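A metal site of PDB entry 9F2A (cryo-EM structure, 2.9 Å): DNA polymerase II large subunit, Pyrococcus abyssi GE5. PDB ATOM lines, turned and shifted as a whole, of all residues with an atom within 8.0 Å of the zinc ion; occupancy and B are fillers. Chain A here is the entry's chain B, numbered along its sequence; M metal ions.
The zinc ion is bound by the side-chain sulfur of Cys 731 (2.3 Å), the side-chain sulfur of Cys 750 (2.3 Å), the side-chain sulfur of Cys 753 (2.3 Å) and the side-chain sulfur of Cys 734 (2.3 Å).
Within 4 Å of the zinc ion: Cys 731, Cys 734, Cys 750 and Cys 753.
The backbone NH of Cys 731 is in hydrogen-bond range of the backbone carbonyl oxygen of Ala 736 (3.4 Å). N of Cys 750 sits at hydrogen-bond distance from O of Val 755.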
ATOM      1  N   VAL A 730      27.265   6.007  -7.943  1.00  0.00           N
ATOM      2  CA  VAL A 730      26.021   5.752  -8.658  1.00  0.00           C
ATOM      3  C   VAL A 730      25.282   4.605  -8.002  1.00  0.00           C
ATOM      4  O   VAL A 730      25.875   3.682  -7.431  1.00  0.00           O
ATOM      5  CB  VAL A 730      26.274   5.450 -10.153  1.00  0.00           C
ATOM      6  CG1 VAL A 730      27.160   6.531 -10.756  1.00  0.00           C
ATOM      7  CG2 VAL A 730      26.905   4.086 -10.328  1.00  0.00           C
ATOM      8  N   CYS A 731      23.948   4.680  -8.054  1.00  0.00           N
ATOM      9  CA  CYS A 731      23.062   3.617  -7.592  1.00  0.00           C
ATOM     10  C   CYS A 731      22.719   2.700  -8.755  1.00  0.00           C
ATOM     11  O   CYS A 731      22.246   3.175  -9.788  1.00  0.00           O
ATOM     12  CB  CYS A 731      21.795   4.197  -6.999  1.00  0.00           C
ATOM     13  SG  CYS A 731      20.690   2.965  -6.278  1.00  0.00           S
ATOM     14  N   PRO A 732      22.949   1.392  -8.631  1.00  0.00           N
ATOM     15  CA  PRO A 732      22.752   0.494  -9.778  1.00  0.00           C
ATOM     16  C   PRO A 732      21.332   0.458 -10.304  1.00  0.00           C
ATOM     17  O   PRO A 732      21.129   0.106 -11.475  1.00  0.00           O
ATOM     18  CB  PRO A 732      23.184  -0.869  -9.245  1.00  0.00           C
ATOM     19  CG  PRO A 732      23.172  -0.740  -7.760  1.00  0.00           C
ATOM     20  CD  PRO A 732      23.497   0.682  -7.466  1.00  0.00           C
ATOM     21  N   ARG A 733      20.328   0.802  -9.491  1.00  0.00           N
ATOM     22  CA  ARG A 733      18.951   0.698  -9.936  1.00  0.00           C
ATOM     23  C   ARG A 733      18.380   2.033 -10.418  1.00  0.00           C
ATOM     24  O   ARG A 733      17.913   2.139 -11.556  1.00  0.00           O
ATOM     25  CB  ARG A 733      18.085   0.124  -8.814  1.00  0.00           C
ATOM     26  CG  ARG A 733      16.592   0.143  -9.112  1.00  0.00           C
ATOM     27  CD  ARG A 733      15.799  -0.528  -8.009  1.00  0.00           C
ATOM     28  NE  ARG A 733      16.282  -1.879  -7.755  1.00  0.00           N
ATOM     29  CZ  ARG A 733      16.652  -2.323  -6.562  1.00  0.00           C
ATOM     30  NH1 ARG A 733      16.604  -1.552  -5.489  1.00  0.00           N
ATOM     31  NH2 ARG A 733      17.074  -3.584  -6.441  1.00  0.00           N
ATOM     32  N   CYS A 734      18.405   3.066  -9.573  1.00  0.00           N
ATOM     33  CA  CYS A 734      17.772   4.329  -9.912  1.00  0.00           C
ATOM     34  C   CYS A 734      18.690   5.292 -10.659  1.00  0.00           C
ATOM     35  O   CYS A 734      18.202   6.299 -11.193  1.00  0.00           O
ATOM     36  CB  CYS A 734      17.246   5.021  -8.653  1.00  0.00           C
ATOM     37  SG  CYS A 734      18.509   5.650  -7.533  1.00  0.00           S
ATOM     38  N   ASN A 735      19.990   5.003 -10.737  1.00  0.00           N
ATOM     39  CA  ASN A 735      20.958   5.819 -11.465  1.00  0.00           C
ATOM     40  C   ASN A 735      20.965   7.263 -10.957  1.00  0.00           C
ATOM     41  O   ASN A 735      20.614   8.210 -11.681  1.00  0.00           O
ATOM     42  CB  ASN A 735      20.695   5.764 -12.975  1.00  0.00           C
ATOM     43  CG  ASN A 735      20.735   4.353 -13.510  1.00  0.00           C
ATOM     44  OD1 ASN A 735      19.941   3.510 -13.107  1.00  0.00           O
ATOM     45  ND2 ASN A 735      21.647   4.101 -14.439  1.00  0.00           N
ATOM     46  N   ALA A 736      21.365   7.422  -9.703  1.00  0.00           N
ATOM     47  CA  ALA A 736      21.502   8.737  -9.088  1.00  0.00           C
ATOM     48  C   ALA A 736      22.960   8.981  -8.723  1.00  0.00           C
ATOM     49  O   ALA A 736      23.677   8.077  -8.293  1.00  0.00           O
ATOM     50  CB  ALA A 736      20.630   8.851  -7.836  1.00  0.00           C
ATOM     51  N   TYR A 738      25.818  10.838  -6.457  1.00  0.00           N
ATOM     52  CA  TYR A 738      26.036  11.383  -5.125  1.00  0.00           C
ATOM     53  C   TYR A 738      27.520  11.716  -4.962  1.00  0.00           C
ATOM     54  O   TYR A 738      28.373  10.849  -5.204  1.00  0.00           O
ATOM     55  CB  TYR A 738      25.597  10.407  -4.033  1.00  0.00           C
ATOM     56  CG  TYR A 738      24.122  10.114  -4.011  1.00  0.00           C
ATOM     57  CD1 TYR A 738      23.203  11.078  -3.611  1.00  0.00           C
ATOM     58  CD2 TYR A 738      23.639   8.869  -4.386  1.00  0.00           C
ATOM     59  CE1 TYR A 738      21.854  10.811  -3.587  1.00  0.00           C
ATOM     60  CE2 TYR A 738      22.286   8.591  -4.369  1.00  0.00           C
ATOM     61  CZ  TYR A 738      21.400   9.559  -3.969  1.00  0.00           C
ATOM     62  OH  TYR A 738      20.056   9.284  -3.948  1.00  0.00           O
ATOM     63  N   THR A 749      24.715   4.093   1.069  1.00  0.00           N
ATOM     64  CA  THR A 749      23.481   3.381   0.771  1.00  0.00           C
ATOM     65  C   THR A 749      22.460   4.370   0.219  1.00  0.00           C
ATOM     66  O   THR A 749      22.309   5.463   0.770  1.00  0.00           O
ATOM     67  CB  THR A 749      22.926   2.668   2.011  1.00  0.00           C
ATOM     68  OG1 THR A 749      23.922   1.775   2.524  1.00  0.00           O
ATOM     69  CG2 THR A 749      21.684   1.878   1.659  1.00  0.00           C
ATOM     70  N   CYS A 750      21.779   3.981  -0.849  1.00  0.00           N
ATOM     71  CA  CYS A 750      20.774   4.844  -1.448  1.00  0.00           C
ATOM     72  C   CYS A 750      19.545   4.897  -0.558  1.00  0.00           C
ATOM     73  O   CYS A 750      18.977   3.836  -0.250  1.00  0.00           O
ATOM     74  CB  CYS A 750      20.413   4.336  -2.847  1.00  0.00           C
ATOM     75  SG  CYS A 750      19.248   5.379  -3.758  1.00  0.00           S
ATOM     76  N   PRO A 751      19.106   6.077  -0.112  1.00  0.00           N
ATOM     77  CA  PRO A 751      17.929   6.125   0.767  1.00  0.00           C
ATOM     78  C   PRO A 751      16.670   5.562   0.133  1.00  0.00           C
ATOM     79  O   PRO A 751      15.853   4.929   0.821  1.00  0.00           O
ATOM     80  CB  PRO A 751      17.797   7.619   1.087  1.00  0.00           C
ATOM     81  CG  PRO A 751      18.490   8.308  -0.035  1.00  0.00           C
ATOM     82  CD  PRO A 751      19.625   7.413  -0.432  1.00  0.00           C
ATOM     83  N   LYS A 752      16.482   5.773  -1.175  1.00  0.00           N
ATOM     84  CA  LYS A 752      15.278   5.297  -1.843  1.00  0.00           C
ATOM     85  C   LYS A 752      15.297   3.788  -2.051  1.00  0.00           C
ATOM     86  O   LYS A 752      14.289   3.107  -1.798  1.00  0.00           O
ATOM     87  CB  LYS A 752      15.098   6.016  -3.178  1.00  0.00           C
ATOM     88  CG  LYS A 752      14.832   7.498  -3.062  1.00  0.00           C
ATOM     89  CD  LYS A 752      14.817   8.147  -4.435  1.00  0.00           C
ATOM     90  CE  LYS A 752      13.604   7.705  -5.237  1.00  0.00           C
ATOM     91  NZ  LYS A 752      13.521   8.402  -6.545  1.00  0.00           N
ATOM     92  N   CYS A 753      16.415   3.250  -2.515  1.00  0.00           N
ATOM     93  CA  CYS A 753      16.487   1.856  -2.928  1.00  0.00           C
ATOM     94  C   CYS A 753      17.006   0.928  -1.848  1.00  0.00           C
ATOM     95  O   CYS A 753      16.784  -0.289  -1.929  1.00  0.00           O
ATOM     96  CB  CYS A 753      17.367   1.706  -4.172  1.00  0.00           C
ATOM     97  SG  CYS A 753      16.944   2.838  -5.515  1.00  0.00           S
ATOM     98  N   ASN A 754      17.700   1.463  -0.841  1.00  0.00           N
ATOM     99  CA  ASN A 754      18.327   0.656   0.215  1.00  0.00           C
ATOM    100  C   ASN A 754      19.249  -0.411  -0.375  1.00  0.00           C
ATOM    101  O   ASN A 754      19.237  -1.569   0.036  1.00  0.00           O
ATOM    102  CB  ASN A 754      17.271   0.032   1.132  1.00  0.00           C
ATOM    103  CG  ASN A 754      17.855  -0.457   2.442  1.00  0.00           C
ATOM    104  OD1 ASN A 754      19.046  -0.322   2.689  1.00  0.00           O
ATOM    105  ND2 ASN A 754      17.000  -1.018   3.295  1.00  0.00           N
ATOM    106  N   VAL A 755      20.060  -0.001  -1.353  1.00  0.00           N
ATOM    107  CA  VAL A 755      21.025  -0.888  -1.990  1.00  0.00           C
ATOM    108  C   VAL A 755      22.409  -0.246  -1.905  1.00  0.00           C
ATOM    109  O   VAL A 755      22.546   0.954  -1.672  1.00  0.00           O
ATOM    110  CB  VAL A 755      20.666  -1.207  -3.453  1.00  0.00           C
ATOM    111  CG1 VAL A 755      19.330  -1.913  -3.523  1.00  0.00           C
ATOM    112  CG2 VAL A 755      20.655   0.061  -4.278  1.00  0.00           C
ATOM    113  N   LYS A 756      23.430  -1.075  -2.093  1.00  0.00           N
ATOM    114  CA  LYS A 756      24.803  -0.614  -1.977  1.00  0.00           C
ATOM    115  C   LYS A 756      25.234   0.134  -3.221  1.00  0.00           C
ATOM    116  O   LYS A 756      24.944  -0.289  -4.349  1.00  0.00           O
ATOM    117  CB  LYS A 756      25.736  -1.804  -1.725  1.00  0.00           C
ATOM    118  CG  LYS A 756      27.143  -1.407  -1.331  1.00  0.00           C
ATOM    119  CD  LYS A 756      27.143  -0.641  -0.027  1.00  0.00           C
ATOM    120  CE  LYS A 756      26.652  -1.499   1.122  1.00  0.00           C
ATOM    121  NZ  LYS A 756      27.604  -2.604   1.422  1.00  0.00           N
ATOM    122  N   LEU A 757      25.916   1.265  -3.035  1.00  0.00           N
ATOM    123  CA  LEU A 757      26.342   2.106  -4.129  1.00  0.00           C
ATOM    124  C   LEU A 757      27.643   1.598  -4.747  1.00  0.00           C
ATOM    125  O   LEU A 757      28.359   0.779  -4.169  1.00  0.00           O
ATOM    126  CB  LEU A 757      26.519   3.549  -3.646  1.00  0.00           C
ATOM    127  CG  LEU A 757      25.304   4.469  -3.731  1.00  0.00           C
ATOM    128  CD1 LEU A 757      24.175   3.933  -2.894  1.00  0.00           C
ATOM    129  CD2 LEU A 757      25.670   5.862  -3.279  1.00  0.00           C
HETATM  130 ZN    ZN M   1      18.813   4.213  -5.720  1.00  0.00          ZN
